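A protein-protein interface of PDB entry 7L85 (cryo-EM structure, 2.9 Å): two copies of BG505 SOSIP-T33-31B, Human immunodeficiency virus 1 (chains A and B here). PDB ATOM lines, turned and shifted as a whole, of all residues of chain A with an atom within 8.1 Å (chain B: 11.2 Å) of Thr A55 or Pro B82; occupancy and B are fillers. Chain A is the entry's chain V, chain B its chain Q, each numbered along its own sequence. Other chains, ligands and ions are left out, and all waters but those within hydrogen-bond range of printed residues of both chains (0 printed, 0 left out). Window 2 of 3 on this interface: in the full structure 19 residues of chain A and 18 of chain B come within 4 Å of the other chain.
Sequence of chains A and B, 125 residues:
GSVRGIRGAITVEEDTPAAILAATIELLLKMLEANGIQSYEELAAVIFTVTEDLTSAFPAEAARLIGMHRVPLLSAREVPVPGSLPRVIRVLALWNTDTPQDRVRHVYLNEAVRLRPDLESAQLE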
ATOM      1  N   GLU A  14     -28.680  27.305  32.990  1.00  0.00           N
ATOM      2  CA  GLU A  14     -27.515  26.450  32.963  1.00  0.00           C
ATOM      3  C   GLU A  14     -27.833  25.056  32.476  1.00  0.00           C
ATOM      4  O   GLU A  14     -28.960  24.580  32.581  1.00  0.00           O
ATOM      5  CB  GLU A  14     -26.862  26.379  34.320  1.00  0.00           C
ATOM      6  CG  GLU A  14     -27.694  25.781  35.370  1.00  0.00           C
ATOM      7  CD  GLU A  14     -26.961  25.714  36.646  1.00  0.00           C
ATOM      8  OE1 GLU A  14     -25.992  26.411  36.794  1.00  0.00           O
ATOM      9  OE2 GLU A  14     -27.345  24.938  37.485  1.00  0.00           O
ATOM     10  N   ASP A  15     -26.819  24.356  31.997  1.00  0.00           N
ATOM     11  CA  ASP A  15     -27.001  23.000  31.516  1.00  0.00           C
ATOM     12  C   ASP A  15     -26.920  21.985  32.642  1.00  0.00           C
ATOM     13  O   ASP A  15     -25.960  21.224  32.749  1.00  0.00           O
ATOM     14  CB  ASP A  15     -25.941  22.693  30.468  1.00  0.00           C
ATOM     15  CG  ASP A  15     -26.166  21.420  29.675  1.00  0.00           C
ATOM     16  OD1 ASP A  15     -27.218  20.809  29.753  1.00  0.00           O
ATOM     17  OD2 ASP A  15     -25.300  21.069  28.915  1.00  0.00           O
ATOM     18  N   THR A  16     -27.936  21.995  33.463  1.00  0.00           N
ATOM     19  CA  THR A  16     -28.086  21.107  34.600  1.00  0.00           C
ATOM     20  C   THR A  16     -29.307  20.261  34.344  1.00  0.00           C
ATOM     21  O   THR A  16     -30.377  20.831  34.139  1.00  0.00           O
ATOM     22  CB  THR A  16     -28.228  21.893  35.903  1.00  0.00           C
ATOM     23  OG1 THR A  16     -27.046  22.629  36.121  1.00  0.00           O
ATOM     24  CG2 THR A  16     -28.482  20.996  37.075  1.00  0.00           C
ATOM     25  N   PRO A  17     -29.249  18.928  34.412  1.00  0.00           N
ATOM     26  CA  PRO A  17     -30.361  18.064  34.140  1.00  0.00           C
ATOM     27  C   PRO A  17     -31.618  18.455  34.855  1.00  0.00           C
ATOM     28  O   PRO A  17     -32.692  18.421  34.271  1.00  0.00           O
ATOM     29  CB  PRO A  17     -29.862  16.743  34.682  1.00  0.00           C
ATOM     30  CG  PRO A  17     -28.414  16.803  34.485  1.00  0.00           C
ATOM     31  CD  PRO A  17     -28.038  18.222  34.784  1.00  0.00           C
ATOM     32  N   ILE A  20     -33.151  21.435  33.047  1.00  0.00           N
ATOM     33  CA  ILE A  20     -33.699  21.098  31.762  1.00  0.00           C
ATOM     34  C   ILE A  20     -35.007  20.417  31.928  1.00  0.00           C
ATOM     35  O   ILE A  20     -35.959  20.711  31.198  1.00  0.00           O
ATOM     36  CB  ILE A  20     -32.748  20.225  30.973  1.00  0.00           C
ATOM     37  CG1 ILE A  20     -31.557  21.057  30.636  1.00  0.00           C
ATOM     38  CG2 ILE A  20     -33.442  19.635  29.723  1.00  0.00           C
ATOM     39  CD1 ILE A  20     -30.420  20.296  30.125  1.00  0.00           C
ATOM     40  N   VAL A  50     -33.129  21.363  20.805  1.00  0.00           N
ATOM     41  CA  VAL A  50     -32.365  22.209  21.697  1.00  0.00           C
ATOM     42  C   VAL A  50     -31.166  22.813  21.060  1.00  0.00           C
ATOM     43  O   VAL A  50     -30.580  22.236  20.135  1.00  0.00           O
ATOM     44  CB  VAL A  50     -31.894  21.445  22.929  1.00  0.00           C
ATOM     45  CG1 VAL A  50     -33.054  20.919  23.689  1.00  0.00           C
ATOM     46  CG2 VAL A  50     -31.013  20.355  22.532  1.00  0.00           C
ATOM     47  N   THR A  51     -30.713  23.887  21.659  1.00  0.00           N
ATOM     48  CA  THR A  51     -29.508  24.526  21.222  1.00  0.00           C
ATOM     49  C   THR A  51     -28.296  23.705  21.582  1.00  0.00           C
ATOM     50  O   THR A  51     -28.333  22.807  22.421  1.00  0.00           O
ATOM     51  CB  THR A  51     -29.462  25.965  21.750  1.00  0.00           C
ATOM     52  OG1 THR A  51     -29.575  25.983  23.172  1.00  0.00           O
ATOM     53  CG2 THR A  51     -30.577  26.731  21.180  1.00  0.00           C
ATOM     54  N   GLU A  52     -27.189  24.038  20.958  1.00  0.00           N
ATOM     55  CA  GLU A  52     -25.951  23.289  21.070  1.00  0.00           C
ATOM     56  C   GLU A  52     -25.312  23.253  22.434  1.00  0.00           C
ATOM     57  O   GLU A  52     -24.445  22.421  22.689  1.00  0.00           O
ATOM     58  CB  GLU A  52     -24.955  23.843  20.050  1.00  0.00           C
ATOM     59  CG  GLU A  52     -24.527  25.288  20.302  1.00  0.00           C
ATOM     60  CD  GLU A  52     -25.501  26.286  19.753  1.00  0.00           C
ATOM     61  OE1 GLU A  52     -26.508  25.871  19.222  1.00  0.00           O
ATOM     62  OE2 GLU A  52     -25.250  27.454  19.858  1.00  0.00           O
ATOM     63  N   ASP A  53     -25.713  24.154  23.297  1.00  0.00           N
ATOM     64  CA  ASP A  53     -25.195  24.273  24.628  1.00  0.00           C
ATOM     65  C   ASP A  53     -25.965  23.543  25.714  1.00  0.00           C
ATOM     66  O   ASP A  53     -25.591  23.659  26.879  1.00  0.00           O
ATOM     67  CB  ASP A  53     -25.086  25.751  24.920  1.00  0.00           C
ATOM     68  CG  ASP A  53     -26.395  26.353  24.698  1.00  0.00           C
ATOM     69  OD1 ASP A  53     -27.261  25.608  24.338  1.00  0.00           O
ATOM     70  OD2 ASP A  53     -26.578  27.531  24.807  1.00  0.00           O
ATOM     71  N   LEU A  54     -26.994  22.776  25.362  1.00  0.00           N
ATOM     72  CA  LEU A  54     -27.688  21.994  26.369  1.00  0.00           C
ATOM     73  C   LEU A  54     -27.546  20.528  26.082  1.00  0.00           C
ATOM     74  O   LEU A  54     -28.286  19.983  25.266  1.00  0.00           O
ATOM     75  CB  LEU A  54     -29.178  22.317  26.431  1.00  0.00           C
ATOM     76  CG  LEU A  54     -29.565  23.726  26.741  1.00  0.00           C
ATOM     77  CD1 LEU A  54     -31.062  23.855  26.629  1.00  0.00           C
ATOM     78  CD2 LEU A  54     -29.118  24.097  28.126  1.00  0.00           C
ATOM     79  N   THR A  55     -26.599  19.871  26.732  1.00  0.00           N
ATOM     80  CA  THR A  55     -26.371  18.471  26.471  1.00  0.00           C
ATOM     81  C   THR A  55     -26.484  17.582  27.696  1.00  0.00           C
ATOM     82  O   THR A  55     -26.197  16.402  27.602  1.00  0.00           O
ATOM     83  CB  THR A  55     -25.020  18.245  25.790  1.00  0.00           C
ATOM     84  OG1 THR A  55     -23.964  18.727  26.623  1.00  0.00           O
ATOM     85  CG2 THR A  55     -24.995  18.990  24.457  1.00  0.00           C
ATOM     86  N   SER A  56     -26.846  18.096  28.861  1.00  0.00           N
ATOM     87  CA  SER A  56     -26.875  17.219  30.029  1.00  0.00           C
ATOM     88  C   SER A  56     -28.111  16.335  30.185  1.00  0.00           C
ATOM     89  O   SER A  56     -28.116  15.427  31.013  1.00  0.00           O
ATOM     90  CB  SER A  56     -26.684  18.020  31.283  1.00  0.00           C
ATOM     91  OG  SER A  56     -27.786  18.815  31.539  1.00  0.00           O
ATOM     92  N   ALA A  57     -29.164  16.588  29.431  1.00  0.00           N
ATOM     93  CA  ALA A  57     -30.389  15.813  29.566  1.00  0.00           C
ATOM     94  C   ALA A  57     -31.232  15.880  28.322  1.00  0.00           C
ATOM     95  O   ALA A  57     -31.086  16.788  27.510  1.00  0.00           O
ATOM     96  CB  ALA A  57     -31.190  16.298  30.742  1.00  0.00           C
ATOM     97  N   PHE A  58     -32.140  14.934  28.171  1.00  0.00           N
ATOM     98  CA  PHE A  58     -33.063  14.977  27.059  1.00  0.00           C
ATOM     99  C   PHE A  58     -34.413  15.510  27.489  1.00  0.00           C
ATOM    100  O   PHE A  58     -35.064  14.880  28.304  1.00  0.00           O
ATOM    101  CB  PHE A  58     -33.357  13.598  26.515  1.00  0.00           C
ATOM    102  CG  PHE A  58     -32.292  12.915  25.850  1.00  0.00           C
ATOM    103  CD1 PHE A  58     -31.609  11.934  26.486  1.00  0.00           C
ATOM    104  CD2 PHE A  58     -31.963  13.232  24.567  1.00  0.00           C
ATOM    105  CE1 PHE A  58     -30.624  11.261  25.844  1.00  0.00           C
ATOM    106  CE2 PHE A  58     -30.976  12.570  23.920  1.00  0.00           C
ATOM    107  CZ  PHE A  58     -30.311  11.581  24.554  1.00  0.00           C
ATOM    108  N   PRO A  59     -34.922  16.614  26.952  1.00  0.00           N
ATOM    109  CA  PRO A  59     -36.219  17.167  27.283  1.00  0.00           C
ATOM    110  C   PRO A  59     -37.340  16.140  27.168  1.00  0.00           C
ATOM    111  O   PRO A  59     -38.271  16.106  27.976  1.00  0.00           O
ATOM    112  CB  PRO A  59     -36.363  18.241  26.234  1.00  0.00           C
ATOM    113  CG  PRO A  59     -34.982  18.651  25.937  1.00  0.00           C
ATOM    114  CD  PRO A  59     -34.171  17.397  26.003  1.00  0.00           C
ATOM    115  N   ARG A  77     -31.086  18.344  17.405  1.00  0.00           N
ATOM    116  CA  ARG A  77     -30.255  19.462  17.781  1.00  0.00           C
ATOM    117  C   ARG A  77     -30.407  20.601  16.771  1.00  0.00           C
ATOM    118  O   ARG A  77     -30.482  20.361  15.562  1.00  0.00           O
ATOM    119  CB  ARG A  77     -28.844  18.956  17.872  1.00  0.00           C
ATOM    120  CG  ARG A  77     -27.884  19.829  18.555  1.00  0.00           C
ATOM    121  CD  ARG A  77     -26.606  19.140  18.671  1.00  0.00           C
ATOM    122  NE  ARG A  77     -25.734  19.768  19.638  1.00  0.00           N
ATOM    123  CZ  ARG A  77     -24.415  19.531  19.751  1.00  0.00           C
ATOM    124  NH1 ARG A  77     -23.834  18.695  18.917  1.00  0.00           N
ATOM    125  NH2 ARG A  77     -23.683  20.132  20.694  1.00  0.00           N
ATOM    126  N   THR B  51     -27.720   9.459  16.021  1.00  0.00           N
ATOM    127  CA  THR B  51     -26.742   9.925  16.957  1.00  0.00           C
ATOM    128  C   THR B  51     -25.515  10.442  16.248  1.00  0.00           C
ATOM    129  O   THR B  51     -25.271  10.175  15.073  1.00  0.00           O
ATOM    130  CB  THR B  51     -26.447   8.833  17.989  1.00  0.00           C
ATOM    131  OG1 THR B  51     -26.022   7.634  17.346  1.00  0.00           O
ATOM    132  CG2 THR B  51     -27.664   8.546  18.760  1.00  0.00           C
ATOM    133  N   GLU B  52     -24.710  11.172  16.986  1.00  0.00           N
ATOM    134  CA  GLU B  52     -23.549  11.864  16.458  1.00  0.00           C
ATOM    135  C   GLU B  52     -22.449  10.995  15.900  1.00  0.00           C
ATOM    136  O   GLU B  52     -21.581  11.484  15.178  1.00  0.00           O
ATOM    137  CB  GLU B  52     -22.982  12.771  17.550  1.00  0.00           C
ATOM    138  CG  GLU B  52     -22.437  12.028  18.769  1.00  0.00           C
ATOM    139  CD  GLU B  52     -23.505  11.664  19.755  1.00  0.00           C
ATOM    140  OE1 GLU B  52     -24.654  11.943  19.483  1.00  0.00           O
ATOM    141  OE2 GLU B  52     -23.191  11.112  20.769  1.00  0.00           O
ATOM    142  N   ASP B  53     -22.465   9.731  16.243  1.00  0.00           N
ATOM    143  CA  ASP B  53     -21.484   8.775  15.820  1.00  0.00           C
ATOM    144  C   ASP B  53     -21.821   7.976  14.574  1.00  0.00           C
ATOM    145  O   ASP B  53     -21.036   7.107  14.203  1.00  0.00           O
ATOM    146  CB  ASP B  53     -21.218   7.876  17.004  1.00  0.00           C
ATOM    147  CG  ASP B  53     -22.491   7.319  17.443  1.00  0.00           C
ATOM    148  OD1 ASP B  53     -23.457   7.665  16.824  1.00  0.00           O
ATOM    149  OD2 ASP B  53     -22.574   6.610  18.402  1.00  0.00           O
ATOM    150  N   ARG B  77     -29.864  15.403  13.019  1.00  0.00           N
ATOM    151  CA  ARG B  77     -28.911  14.857  13.952  1.00  0.00           C
ATOM    152  C   ARG B  77     -29.385  15.083  15.389  1.00  0.00           C
ATOM    153  O   ARG B  77     -29.914  16.150  15.716  1.00  0.00           O
ATOM    154  CB  ARG B  77     -27.589  15.511  13.672  1.00  0.00           C
ATOM    155  CG  ARG B  77     -26.410  14.874  14.271  1.00  0.00           C
ATOM    156  CD  ARG B  77     -25.208  15.547  13.798  1.00  0.00           C
ATOM    157  NE  ARG B  77     -24.015  14.768  14.040  1.00  0.00           N
ATOM    158  CZ  ARG B  77     -22.760  15.244  13.973  1.00  0.00           C
ATOM    159  NH1 ARG B  77     -22.563  16.516  13.699  1.00  0.00           N
ATOM    160  NH2 ARG B  77     -21.706  14.447  14.179  1.00  0.00           N
ATOM    161  N   GLU B  78     -29.186  14.078  16.240  1.00  0.00           N
ATOM    162  CA  GLU B  78     -29.590  14.075  17.652  1.00  0.00           C
ATOM    163  C   GLU B  78     -28.660  14.776  18.603  1.00  0.00           C
ATOM    164  O   GLU B  78     -27.473  14.931  18.339  1.00  0.00           O
ATOM    165  CB  GLU B  78     -29.754  12.687  18.175  1.00  0.00           C
ATOM    166  CG  GLU B  78     -30.795  11.952  17.522  1.00  0.00           C
ATOM    167  CD  GLU B  78     -30.971  10.663  18.105  1.00  0.00           C
ATOM    168  OE1 GLU B  78     -30.398  10.416  19.149  1.00  0.00           O
ATOM    169  OE2 GLU B  78     -31.670   9.850  17.546  1.00  0.00           O
ATOM    170  N   VAL B  79     -29.209  15.133  19.750  1.00  0.00           N
ATOM    171  CA  VAL B  79     -28.488  15.782  20.818  1.00  0.00           C
ATOM    172  C   VAL B  79     -27.570  14.789  21.533  1.00  0.00           C
ATOM    173  O   VAL B  79     -28.066  13.829  22.117  1.00  0.00           O
ATOM    174  CB  VAL B  79     -29.488  16.286  21.842  1.00  0.00           C
ATOM    175  CG1 VAL B  79     -28.765  16.949  23.011  1.00  0.00           C
ATOM    176  CG2 VAL B  79     -30.451  17.204  21.175  1.00  0.00           C
ATOM    177  N   PRO B  80     -26.265  15.043  21.629  1.00  0.00           N
ATOM    178  CA  PRO B  80     -25.262  14.180  22.209  1.00  0.00           C
ATOM    179  C   PRO B  80     -25.227  14.202  23.718  1.00  0.00           C
ATOM    180  O   PRO B  80     -24.269  14.698  24.300  1.00  0.00           O
ATOM    181  CB  PRO B  80     -23.986  14.773  21.653  1.00  0.00           C
ATOM    182  CG  PRO B  80     -24.279  16.205  21.543  1.00  0.00           C
ATOM    183  CD  PRO B  80     -25.718  16.274  21.113  1.00  0.00           C
ATOM    184  N   VAL B  81     -26.270  13.716  24.349  1.00  0.00           N
ATOM    185  CA  VAL B  81     -26.289  13.694  25.800  1.00  0.00           C
ATOM    186  C   VAL B  81     -25.354  12.595  26.295  1.00  0.00           C
ATOM    187  O   VAL B  81     -25.512  11.452  25.869  1.00  0.00           O
ATOM    188  CB  VAL B  81     -27.696  13.422  26.328  1.00  0.00           C
ATOM    189  CG1 VAL B  81     -27.705  13.298  27.813  1.00  0.00           C
ATOM    190  CG2 VAL B  81     -28.600  14.534  25.929  1.00  0.00           C
ATOM    191  N   PRO B  82     -24.373  12.872  27.158  1.00  0.00           N
ATOM    192  CA  PRO B  82     -23.443  11.903  27.664  1.00  0.00           C
ATOM    193  C   PRO B  82     -24.186  10.795  28.336  1.00  0.00           C
ATOM    194  O   PRO B  82     -25.146  11.045  29.053  1.00  0.00           O
ATOM    195  CB  PRO B  82     -22.658  12.696  28.690  1.00  0.00           C
ATOM    196  CG  PRO B  82     -22.763  14.096  28.221  1.00  0.00           C
ATOM    197  CD  PRO B  82     -24.135  14.211  27.643  1.00  0.00           C
ATOM    198  N   GLY B  83     -23.740   9.578  28.131  1.00  0.00           N
ATOM    199  CA  GLY B  83     -24.376   8.440  28.758  1.00  0.00           C
ATOM    200  C   GLY B  83     -25.491   7.843  27.915  1.00  0.00           C
ATOM    201  O   GLY B  83     -26.037   6.798  28.270  1.00  0.00           O
ATOM    202  N   SER B  84     -25.827   8.477  26.802  1.00  0.00           N
ATOM    203  CA  SER B  84     -26.883   7.962  25.967  1.00  0.00           C
ATOM    204  C   SER B  84     -26.426   6.716  25.250  1.00  0.00           C
ATOM    205  O   SER B  84     -25.233   6.429  25.146  1.00  0.00           O
ATOM    206  CB  SER B  84     -27.299   9.001  24.969  1.00  0.00           C
ATOM    207  OG  SER B  84     -26.286   9.217  24.035  1.00  0.00           O
ATOM    208  N   LEU B  85     -27.380   5.960  24.743  1.00  0.00           N
ATOM    209  CA  LEU B  85     -27.073   4.768  23.992  1.00  0.00           C
ATOM    210  C   LEU B  85     -26.428   5.208  22.667  1.00  0.00           C
ATOM    211  O   LEU B  85     -27.007   6.055  21.993  1.00  0.00           O
ATOM    212  CB  LEU B  85     -28.388   4.020  23.752  1.00  0.00           C
ATOM    213  CG  LEU B  85     -28.351   2.654  23.095  1.00  0.00           C
ATOM    214  CD1 LEU B  85     -27.707   1.660  23.993  1.00  0.00           C
ATOM    215  CD2 LEU B  85     -29.756   2.206  22.804  1.00  0.00           C
ATOM    216  N   PRO B  86     -25.228   4.732  22.301  1.00  0.00           N
ATOM    217  CA  PRO B  86     -24.493   5.062  21.098  1.00  0.00           C
ATOM    218  C   PRO B  86     -25.052   4.391  19.873  1.00  0.00           C
ATOM    219  O   PRO B  86     -25.721   3.370  19.984  1.00  0.00           O
ATOM    220  CB  PRO B  86     -23.108   4.539  21.415  1.00  0.00           C
ATOM    221  CG  PRO B  86     -23.353   3.401  22.317  1.00  0.00           C
ATOM    222  CD  PRO B  86     -24.532   3.798  23.144  1.00  0.00           C
ATOM    223  N   ARG B  90     -33.186   6.472  15.050  1.00  0.00           N
ATOM    224  CA  ARG B  90     -34.556   6.598  15.526  1.00  0.00           C
ATOM    225  C   ARG B  90     -35.457   7.063  14.424  1.00  0.00           C
ATOM    226  O   ARG B  90     -35.083   7.906  13.615  1.00  0.00           O
ATOM    227  CB  ARG B  90     -34.673   7.581  16.654  1.00  0.00           C
ATOM    228  CG  ARG B  90     -34.007   7.211  17.918  1.00  0.00           C
ATOM    229  CD  ARG B  90     -34.227   8.241  18.923  1.00  0.00           C
ATOM    230  NE  ARG B  90     -33.795   7.865  20.262  1.00  0.00           N
ATOM    231  CZ  ARG B  90     -32.541   7.938  20.715  1.00  0.00           C
ATOM    232  NH1 ARG B  90     -31.604   8.294  19.925  1.00  0.00           N
ATOM    233  NH2 ARG B  90     -32.279   7.664  21.967  1.00  0.00           N
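The backbone carbonyl oxygen (O) of Arg B77 lies within hydrogen-bond range of the backbone NH (N) of Arg A77, 3.0 Å away.
NH2 of Arg B77 sits at hydrogen-bond distance from O of Glu B52 (3.1 Å).
OG of Ser B84 lies within hydrogen-bond range of O of Val B81.
OD2 of Asp A15 lies within hydrogen-bond range of N of Thr A55, at 2.8 Å.
OD1 of Asp A15 lies within hydrogen-bond range of OG of Ser A56 (2.7 Å).
The backbone carbonyl oxygen (O) of Glu A52 sits at hydrogen-bond distance from the guanidinium group (NH2) of Arg A77, 3.1 Å away.
CG2 of Val A50 touches CG2 of Val B79 (3.5 Å).
Val B79 touches Leu A54.
Thr A55 touches Pro B80.
Thr A55 touches Val B81.
Pro B82 touches Thr A55 (CD to O, 3.0 Å).
Ser A56 touches Val B81.
Val B79 touches Phe A58 (O to CE2, 3.6 Å).
Phe A58 touches Val B81.
Arg A77 touches Val B79 (N to CG2, 3.99 Å).
Arg A77 touches Pro B80 (NH1 to CG, 3.6 Å).
No residue of chain B comes within 4 Å of Asp A15.
Of the printed residues of chain B, Leu A54 touches Val B79.
Ser A56 touches just one residue of chain B: Val B81.
Val B81 touches just these residues of chain A: Thr A55 (3.3 Å), Ser A56 (3.9 Å), Ala A57 (3.7 Å) and Phe A58 (3.7 Å).
Of the printed residues of chain A, Ser B84 touches Phe A58.
Printed residues of chain A within 4 Å of Arg B77: Arg A77 (3.0 Å).
Printed residues of chain A within 4 Å of Pro B80: Thr A55 (3.9 Å) and Arg A77 (3.6 Å).
Of the printed residues of chain B, Phe A58 touches Val B79 (3.6 Å), Val B81 (3.7 Å) and Ser B84 (3.99 Å).
The nearest residue of chain A that does not touch Pro B82 is Ser A56 (4.7 Å).
The nearest printed residue of chain A that does not touch Arg B77 is Val A50 (7.6 Å).
Of the 16 printed residues of chain A, 7 touch a printed residue of chain B.
Hydrophobic or aromatic side chains of chain A within 4 Å of the printed part of chain B: Val A50 and Phe A58.
Among the printed residues, no Asp or Glu carboxylate lies within 4 Å of a Lys or Arg side-chain nitrogen of the other chain.
Arg B77 touches its own counterpart, Arg A77.
Positions printed for both chains: 51, 52, 53 and 77.
Of the 13 pairs that touch across the chains among the printed residues, 1 has its exchanged pair printed and touching as well.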
